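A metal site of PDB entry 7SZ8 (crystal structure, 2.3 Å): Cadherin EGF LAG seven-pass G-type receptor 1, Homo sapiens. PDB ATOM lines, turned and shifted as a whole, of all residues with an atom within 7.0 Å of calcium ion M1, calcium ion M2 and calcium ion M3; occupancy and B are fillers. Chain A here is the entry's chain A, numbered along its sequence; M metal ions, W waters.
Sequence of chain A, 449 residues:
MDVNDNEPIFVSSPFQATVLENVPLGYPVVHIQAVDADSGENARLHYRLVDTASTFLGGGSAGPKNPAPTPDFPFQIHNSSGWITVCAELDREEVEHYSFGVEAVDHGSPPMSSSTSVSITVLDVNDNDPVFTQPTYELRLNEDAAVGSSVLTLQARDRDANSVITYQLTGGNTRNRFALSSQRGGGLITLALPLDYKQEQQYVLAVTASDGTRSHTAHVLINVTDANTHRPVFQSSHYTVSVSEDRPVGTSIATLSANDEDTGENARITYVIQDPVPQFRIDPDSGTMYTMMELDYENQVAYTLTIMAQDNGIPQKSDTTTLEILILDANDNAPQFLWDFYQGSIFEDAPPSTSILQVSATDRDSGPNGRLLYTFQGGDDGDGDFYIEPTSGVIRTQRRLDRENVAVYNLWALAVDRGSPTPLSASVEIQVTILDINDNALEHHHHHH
Calcium ion M3 is bound by the side-chain amide oxygen (OD1) of Asn 126. O of Asn 128 is bound to calcium ion M3, at 2.3 Å. The side-chain carboxylate (OD2) of Asp 158 is bound to calcium ion M3, at 2.3 Å. The side-chain carboxylate (OD1) of Asp 158 is bound to calcium ion M3 (2.4 Å). OD2 of Asp 211 is bound to calcium ion M3 (2.5 Å). OD2 of Asp 160 binds calcium ion M3 (2.6 Å). The side-chain hydroxyl (OG) of Ser 163 is bound to calcium ion M3, at 2.7 Å. Calcium ion M3 has seven donor atoms within binding distance.
Calcium ion M2 is bound by the side-chain carboxylate (OD1) of Asp 160 (2.0 Å), the side-chain carboxylate (OE2) of Glu 93 (2.3 Å), the side-chain carboxylate (OE2) of Glu 21 (2.3 Å), the backbone carbonyl oxygen (O) of Val 125 (2.4 Å), the side-chain carboxylate (OD1) of Asp 127 (2.5 Å), the side-chain carboxylate (OD1) of Asp 124 (2.6 Å) and the side-chain carboxylate (OE1) of Glu 93 (2.8 Å). Calcium ion M2 has seven donor atoms within binding distance.
Within 4 Å of calcium ion M2: Glu 21, Glu 93, Asp 124, Val 125, Asp 127 and Asp 160. The nearest printed residue that does not touch calcium ion M2 is Asn 128 (4.1 Å).
The backbone NH (N) of Asn 162 lies within hydrogen-bond range of the side-chain carboxylate (OD2) of Asp 124, 3.5 Å away. N of Arg 92 sits close to OE1 of Glu 21 (2.8 Å). OD1 of Asp 211 is in hydrogen-bond range of N of Thr 213 (2.8 Å). The side-chain amide oxygen (OD1) of Asn 128 lies within hydrogen-bond range of the guanidinium group (NH1) of Arg 159 (2.7 Å). The backbone NH (N) of Arg 214 sits at hydrogen-bond distance from the side-chain carboxylate (OD1) of Asp 211, 2.7 Å away. O of Leu 123 is in hydrogen-bond range of N of Glu 21 (3.0 Å). The side-chain carboxylate (OE1) of Glu 93 sits close to the side-chain amide nitrogen (ND2) of Asn 128, at 3.3 Å. OD1 of Asp 127 sits close to ND2 of Asn 128, at 3.1 Å.
Calcium ion M1 is bound by OE1 of Glu 21, OE1 of Glu 93, OD1 of Asp 91, OD2 of Asp 127, water W2 and water W1.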
ATOM      1  N   GLU A  21     -16.495  -9.351  -6.627  1.00  0.00           N
ATOM      2  CA  GLU A  21     -15.620  -9.251  -5.427  1.00  0.00           C
ATOM      3  C   GLU A  21     -16.226  -8.286  -4.400  1.00  0.00           C
ATOM      4  O   GLU A  21     -15.721  -8.219  -3.293  1.00  0.00           O
ATOM      5  CB  GLU A  21     -14.200  -8.841  -5.801  1.00  0.00           C
ATOM      6  CG  GLU A  21     -14.028  -7.385  -6.262  1.00  0.00           C
ATOM      7  CD  GLU A  21     -12.558  -7.037  -6.423  1.00  0.00           C
ATOM      8  OE1 GLU A  21     -11.718  -7.423  -5.549  1.00  0.00           O
ATOM      9  OE2 GLU A  21     -12.221  -6.464  -7.471  1.00  0.00           O
ATOM     10  N   LEU A  90     -14.919 -10.325  -0.081  1.00  0.00           N
ATOM     11  CA  LEU A  90     -14.132 -10.990  -1.154  1.00  0.00           C
ATOM     12  C   LEU A  90     -13.098  -9.984  -1.675  1.00  0.00           C
ATOM     13  O   LEU A  90     -13.268  -8.774  -1.408  1.00  0.00           O
ATOM     14  CB  LEU A  90     -15.089 -11.387  -2.269  1.00  0.00           C
ATOM     15  CG  LEU A  90     -16.145 -12.421  -1.922  1.00  0.00           C
ATOM     16  CD1 LEU A  90     -16.842 -12.886  -3.198  1.00  0.00           C
ATOM     17  CD2 LEU A  90     -15.533 -13.580  -1.181  1.00  0.00           C
ATOM     18  N   ASP A  91     -12.069 -10.456  -2.390  1.00  0.00           N
ATOM     19  CA  ASP A  91     -11.047  -9.576  -3.005  1.00  0.00           C
ATOM     20  C   ASP A  91     -10.389 -10.325  -4.155  1.00  0.00           C
ATOM     21  O   ASP A  91      -9.561 -11.163  -3.894  1.00  0.00           O
ATOM     22  CB  ASP A  91     -10.044  -9.110  -1.939  1.00  0.00           C
ATOM     23  CG  ASP A  91      -8.930  -8.199  -2.449  1.00  0.00           C
ATOM     24  OD1 ASP A  91      -8.996  -7.756  -3.586  1.00  0.00           O
ATOM     25  OD2 ASP A  91      -8.030  -7.919  -1.671  1.00  0.00           O
ATOM     26  N   ARG A  92     -10.734 -10.001  -5.400  1.00  0.00           N
ATOM     27  CA  ARG A  92     -10.191 -10.733  -6.571  1.00  0.00           C
ATOM     28  C   ARG A  92      -8.661 -10.577  -6.615  1.00  0.00           C
ATOM     29  O   ARG A  92      -8.002 -11.499  -7.059  1.00  0.00           O
ATOM     30  CB  ARG A  92     -10.802 -10.239  -7.893  1.00  0.00           C
ATOM     31  CG  ARG A  92     -10.495 -11.205  -9.031  1.00  0.00           C
ATOM     32  CD  ARG A  92     -10.349 -10.548 -10.370  1.00  0.00           C
ATOM     33  NE  ARG A  92      -9.404  -9.443 -10.285  1.00  0.00           N
ATOM     34  CZ  ARG A  92      -8.146  -9.472 -10.656  1.00  0.00           C
ATOM     35  NH1 ARG A  92      -7.603 -10.584 -11.140  1.00  0.00           N
ATOM     36  NH2 ARG A  92      -7.429  -8.370 -10.497  1.00  0.00           N
ATOM     37  N   GLU A  93      -8.142  -9.473  -6.090  1.00  0.00           N
ATOM     38  CA  GLU A  93      -6.688  -9.186  -6.067  1.00  0.00           C
ATOM     39  C   GLU A  93      -5.974 -10.028  -4.995  1.00  0.00           C
ATOM     40  O   GLU A  93      -4.754 -10.053  -5.028  1.00  0.00           O
ATOM     41  CB  GLU A  93      -6.431  -7.695  -5.879  1.00  0.00           C
ATOM     42  CG  GLU A  93      -6.740  -6.898  -7.122  1.00  0.00           C
ATOM     43  CD  GLU A  93      -8.225  -6.593  -7.319  1.00  0.00           C
ATOM     44  OE1 GLU A  93      -8.885  -6.162  -6.341  1.00  0.00           O
ATOM     45  OE2 GLU A  93      -8.712  -6.774  -8.468  1.00  0.00           O
ATOM     46  N   GLU A  94      -6.718 -10.731  -4.133  1.00  0.00           N
ATOM     47  CA  GLU A  94      -6.173 -11.706  -3.156  1.00  0.00           C
ATOM     48  C   GLU A  94      -6.318 -13.128  -3.706  1.00  0.00           C
ATOM     49  O   GLU A  94      -5.367 -13.865  -3.661  1.00  0.00           O
ATOM     50  CB  GLU A  94      -6.915 -11.613  -1.819  1.00  0.00           C
ATOM     51  CG  GLU A  94      -6.207 -12.353  -0.681  1.00  0.00           C
ATOM     52  CD  GLU A  94      -5.014 -11.611  -0.093  1.00  0.00           C
ATOM     53  OE1 GLU A  94      -3.990 -12.271   0.187  1.00  0.00           O
ATOM     54  OE2 GLU A  94      -5.116 -10.389   0.109  1.00  0.00           O
ATOM     55  N   LEU A 123     -15.267 -12.260  -9.622  1.00  0.00           N
ATOM     56  CA  LEU A 123     -15.283 -11.319 -10.788  1.00  0.00           C
ATOM     57  C   LEU A 123     -14.711  -9.970 -10.373  1.00  0.00           C
ATOM     58  O   LEU A 123     -15.002  -9.523  -9.200  1.00  0.00           O
ATOM     59  CB  LEU A 123     -16.717 -11.197 -11.323  1.00  0.00           C
ATOM     60  CG  LEU A 123     -17.262 -12.469 -11.980  1.00  0.00           C
ATOM     61  CD1 LEU A 123     -18.659 -12.257 -12.525  1.00  0.00           C
ATOM     62  CD2 LEU A 123     -16.325 -12.980 -13.073  1.00  0.00           C
ATOM     63  N   ASP A 124     -13.934  -9.353 -11.258  1.00  0.00           N
ATOM     64  CA  ASP A 124     -13.165  -8.112 -11.007  1.00  0.00           C
ATOM     65  C   ASP A 124     -14.103  -6.918 -11.034  1.00  0.00           C
ATOM     66  O   ASP A 124     -14.944  -6.872 -11.932  1.00  0.00           O
ATOM     67  CB  ASP A 124     -12.107  -7.788 -12.054  1.00  0.00           C
ATOM     68  CG  ASP A 124     -11.131  -6.688 -11.644  1.00  0.00           C
ATOM     69  OD1 ASP A 124     -10.545  -6.834 -10.550  1.00  0.00           O
ATOM     70  OD2 ASP A 124     -10.904  -5.734 -12.458  1.00  0.00           O
ATOM     71  N   VAL A 125     -13.923  -6.023 -10.047  1.00  0.00           N
ATOM     72  CA  VAL A 125     -14.486  -4.641  -9.954  1.00  0.00           C
ATOM     73  C   VAL A 125     -13.286  -3.666  -9.936  1.00  0.00           C
ATOM     74  O   VAL A 125     -12.130  -4.079  -9.584  1.00  0.00           O
ATOM     75  CB  VAL A 125     -15.328  -4.531  -8.670  1.00  0.00           C
ATOM     76  CG1 VAL A 125     -15.513  -3.105  -8.214  1.00  0.00           C
ATOM     77  CG2 VAL A 125     -16.663  -5.244  -8.795  1.00  0.00           C
ATOM     78  N   ASN A 126     -13.510  -2.410 -10.317  1.00  0.00           N
ATOM     79  CA  ASN A 126     -12.448  -1.380 -10.387  1.00  0.00           C
ATOM     80  C   ASN A 126     -12.316  -0.701  -9.009  1.00  0.00           C
ATOM     81  O   ASN A 126     -12.961   0.339  -8.781  1.00  0.00           O
ATOM     82  CB  ASN A 126     -12.707  -0.388 -11.532  1.00  0.00           C
ATOM     83  CG  ASN A 126     -11.513   0.514 -11.707  1.00  0.00           C
ATOM     84  OD1 ASN A 126     -10.423   0.204 -11.258  1.00  0.00           O
ATOM     85  ND2 ASN A 126     -11.697   1.627 -12.398  1.00  0.00           N
ATOM     86  N   ASP A 127     -11.540  -1.310  -8.119  1.00  0.00           N
ATOM     87  CA  ASP A 127     -11.433  -0.900  -6.694  1.00  0.00           C
ATOM     88  C   ASP A 127      -9.965  -0.569  -6.411  1.00  0.00           C
ATOM     89  O   ASP A 127      -9.671  -0.296  -5.244  1.00  0.00           O
ATOM     90  CB  ASP A 127     -12.099  -1.923  -5.738  1.00  0.00           C
ATOM     91  CG  ASP A 127     -11.556  -3.350  -5.770  1.00  0.00           C
ATOM     92  OD1 ASP A 127     -10.739  -3.643  -6.646  1.00  0.00           O
ATOM     93  OD2 ASP A 127     -11.937  -4.179  -4.855  1.00  0.00           O
ATOM     94  N   ASN A 128      -9.094  -0.512  -7.429  1.00  0.00           N
ATOM     95  CA  ASN A 128      -7.698  -0.066  -7.224  1.00  0.00           C
ATOM     96  C   ASN A 128      -7.345   1.083  -8.172  1.00  0.00           C
ATOM     97  O   ASN A 128      -7.659   0.973  -9.394  1.00  0.00           O
ATOM     98  CB  ASN A 128      -6.678  -1.187  -7.408  1.00  0.00           C
ATOM     99  CG  ASN A 128      -6.755  -2.192  -6.277  1.00  0.00           C
ATOM    100  OD1 ASN A 128      -5.958  -2.148  -5.348  1.00  0.00           O
ATOM    101  ND2 ASN A 128      -7.707  -3.104  -6.360  1.00  0.00           N
ATOM    102  N   ASP A 129      -6.689   2.104  -7.610  1.00  0.00           N
ATOM    103  CA  ASP A 129      -6.040   3.220  -8.339  1.00  0.00           C
ATOM    104  C   ASP A 129      -4.809   2.681  -9.089  1.00  0.00           C
ATOM    105  O   ASP A 129      -4.102   1.812  -8.565  1.00  0.00           O
ATOM    106  CB  ASP A 129      -5.603   4.362  -7.414  1.00  0.00           C
ATOM    107  CG  ASP A 129      -6.710   5.067  -6.641  1.00  0.00           C
ATOM    108  OD1 ASP A 129      -7.914   4.778  -6.872  1.00  0.00           O
ATOM    109  OD2 ASP A 129      -6.375   5.900  -5.773  1.00  0.00           O
ATOM    110  N   PRO A 130      -4.468   3.214 -10.281  1.00  0.00           N
ATOM    111  CA  PRO A 130      -3.146   2.984 -10.882  1.00  0.00           C
ATOM    112  C   PRO A 130      -2.059   3.568  -9.980  1.00  0.00           C
ATOM    113  O   PRO A 130      -2.294   4.602  -9.356  1.00  0.00           O
ATOM    114  CB  PRO A 130      -3.164   3.753 -12.219  1.00  0.00           C
ATOM    115  CG  PRO A 130      -4.646   3.985 -12.492  1.00  0.00           C
ATOM    116  CD  PRO A 130      -5.270   4.117 -11.108  1.00  0.00           C
ATOM    117  N   ASP A 158      -1.903  -1.331 -12.480  1.00  0.00           N
ATOM    118  CA  ASP A 158      -3.253  -1.440 -11.878  1.00  0.00           C
ATOM    119  C   ASP A 158      -3.430  -2.916 -11.560  1.00  0.00           C
ATOM    120  O   ASP A 158      -3.378  -3.732 -12.511  1.00  0.00           O
ATOM    121  CB  ASP A 158      -4.335  -0.937 -12.832  1.00  0.00           C
ATOM    122  CG  ASP A 158      -5.610  -0.459 -12.141  1.00  0.00           C
ATOM    123  OD1 ASP A 158      -6.113  -1.165 -11.263  1.00  0.00           O
ATOM    124  OD2 ASP A 158      -6.122   0.633 -12.525  1.00  0.00           O
ATOM    125  N   ARG A 159      -3.640  -3.238 -10.277  1.00  0.00           N
ATOM    126  CA  ARG A 159      -3.862  -4.616  -9.789  1.00  0.00           C
ATOM    127  C   ARG A 159      -5.194  -5.168 -10.275  1.00  0.00           C
ATOM    128  O   ARG A 159      -5.385  -6.338 -10.174  1.00  0.00           O
ATOM    129  CB  ARG A 159      -3.805  -4.638  -8.265  1.00  0.00           C
ATOM    130  CG  ARG A 159      -2.416  -4.347  -7.707  1.00  0.00           C
ATOM    131  CD  ARG A 159      -2.452  -4.014  -6.227  1.00  0.00           C
ATOM    132  NE  ARG A 159      -2.765  -5.171  -5.400  1.00  0.00           N
ATOM    133  CZ  ARG A 159      -3.797  -5.258  -4.539  1.00  0.00           C
ATOM    134  NH1 ARG A 159      -4.668  -4.274  -4.363  1.00  0.00           N
ATOM    135  NH2 ARG A 159      -3.913  -6.364  -3.819  1.00  0.00           N
ATOM    136  N   ASP A 160      -6.121  -4.350 -10.778  1.00  0.00           N
ATOM    137  CA  ASP A 160      -7.351  -4.850 -11.434  1.00  0.00           C
ATOM    138  C   ASP A 160      -6.938  -5.531 -12.760  1.00  0.00           C
ATOM    139  O   ASP A 160      -6.091  -5.001 -13.479  1.00  0.00           O
ATOM    140  CB  ASP A 160      -8.375  -3.717 -11.462  1.00  0.00           C
ATOM    141  CG  ASP A 160      -8.777  -3.134 -10.093  1.00  0.00           C
ATOM    142  OD1 ASP A 160      -9.163  -3.939  -9.200  1.00  0.00           O
ATOM    143  OD2 ASP A 160      -8.735  -1.881  -9.932  1.00  0.00           O
ATOM    144  N   ALA A 161      -7.497  -6.684 -13.131  1.00  0.00           N
ATOM    145  CA  ALA A 161      -7.247  -7.347 -14.443  1.00  0.00           C
ATOM    146  C   ALA A 161      -7.881  -6.523 -15.587  1.00  0.00           C
ATOM    147  O   ALA A 161      -7.331  -6.491 -16.669  1.00  0.00           O
ATOM    148  CB  ALA A 161      -7.795  -8.754 -14.434  1.00  0.00           C
ATOM    149  N   ASN A 162      -8.959  -5.801 -15.320  1.00  0.00           N
ATOM    150  CA  ASN A 162      -9.813  -5.191 -16.380  1.00  0.00           C
ATOM    151  C   ASN A 162      -9.535  -3.683 -16.474  1.00  0.00           C
ATOM    152  O   ASN A 162     -10.443  -2.934 -16.937  1.00  0.00           O
ATOM    153  CB  ASN A 162     -11.294  -5.481 -16.123  1.00  0.00           C
ATOM    154  CG  ASN A 162     -11.582  -6.969 -15.988  1.00  0.00           C
ATOM    155  OD1 ASN A 162     -10.970  -7.812 -16.651  1.00  0.00           O
ATOM    156  ND2 ASN A 162     -12.542  -7.286 -15.156  1.00  0.00           N
ATOM    157  N   SER A 163      -8.326  -3.268 -16.133  1.00  0.00           N
ATOM    158  CA  SER A 163      -7.903  -1.843 -16.072  1.00  0.00           C
ATOM    159  C   SER A 163      -6.799  -1.637 -17.104  1.00  0.00           C
ATOM    160  O   SER A 163      -5.762  -2.233 -16.920  1.00  0.00           O
ATOM    161  CB  SER A 163      -7.503  -1.453 -14.640  1.00  0.00           C
ATOM    162  OG  SER A 163      -8.648  -1.266 -13.780  1.00  0.00           O
ATOM    163  N   VAL A 164      -7.108  -0.902 -18.194  1.00  0.00           N
ATOM    164  CA  VAL A 164      -6.227  -0.274 -19.222  1.00  0.00           C
ATOM    165  C   VAL A 164      -5.762   1.093 -18.710  1.00  0.00           C
ATOM    166  O   VAL A 164      -6.638   1.914 -18.321  1.00  0.00           O
ATOM    167  CB  VAL A 164      -6.987  -0.028 -20.548  1.00  0.00           C
ATOM    168  CG1 VAL A 164      -6.037   0.286 -21.683  1.00  0.00           C
ATOM    169  CG2 VAL A 164      -7.955  -1.148 -20.923  1.00  0.00           C
ATOM    170  N   ASP A 211      -7.255   4.653 -15.306  1.00  0.00           N
ATOM    171  CA  ASP A 211      -7.884   3.411 -15.798  1.00  0.00           C
ATOM    172  C   ASP A 211      -9.224   3.765 -16.481  1.00  0.00           C
ATOM    173  O   ASP A 211      -9.947   2.850 -16.860  1.00  0.00           O
ATOM    174  CB  ASP A 211      -8.065   2.407 -14.677  1.00  0.00           C
ATOM    175  CG  ASP A 211      -8.959   2.869 -13.545  1.00  0.00           C
ATOM    176  OD1 ASP A 211      -9.754   3.792 -13.791  1.00  0.00           O
ATOM    177  OD2 ASP A 211      -8.856   2.287 -12.423  1.00  0.00           O
ATOM    178  N   THR A 213     -11.491   5.673 -14.878  1.00  0.00           N
ATOM    179  CA  THR A 213     -12.342   6.220 -13.784  1.00  0.00           C
ATOM    180  C   THR A 213     -11.467   6.667 -12.592  1.00  0.00           C
ATOM    181  O   THR A 213     -11.782   7.707 -12.048  1.00  0.00           O
ATOM    182  CB  THR A 213     -13.512   5.293 -13.426  1.00  0.00           C
ATOM    183  OG1 THR A 213     -13.095   4.296 -12.508  1.00  0.00           O
ATOM    184  CG2 THR A 213     -14.103   4.537 -14.582  1.00  0.00           C
ATOM    185  N   ARG A 214     -10.422   5.908 -12.226  1.00  0.00           N
ATOM    186  CA  ARG A 214      -9.491   6.212 -11.109  1.00  0.00           C
ATOM    187  C   ARG A 214      -8.130   6.635 -11.644  1.00  0.00           C
ATOM    188  O   ARG A 214      -7.660   6.055 -12.703  1.00  0.00           O
ATOM    189  CB  ARG A 214      -9.234   4.979 -10.257  1.00  0.00           C
ATOM    190  CG  ARG A 214     -10.490   4.445  -9.597  1.00  0.00           C
ATOM    191  CD  ARG A 214     -10.212   3.053  -9.116  1.00  0.00           C
ATOM    192  NE  ARG A 214     -11.263   2.721  -8.186  1.00  0.00           N
ATOM    193  CZ  ARG A 214     -11.247   3.001  -6.904  1.00  0.00           C
ATOM    194  NH1 ARG A 214     -10.220   3.618  -6.347  1.00  0.00           N
ATOM    195  NH2 ARG A 214     -12.273   2.591  -6.184  1.00  0.00           N
HETATM  196 CA    CA M   1     -10.381  -6.042  -4.562  1.00  0.00          CA
HETATM  197 CA    CA M   2     -10.458  -5.306  -8.441  1.00  0.00          CA
HETATM  198 CA    CA M   3      -8.170   0.111 -11.510  1.00  0.00          CA
HETATM  199  O   HOH W   1     -11.512  -5.836  -2.356  1.00  0.00           O
HETATM  200  O   HOH W   2      -8.836  -4.348  -3.665  1.00  0.00           O
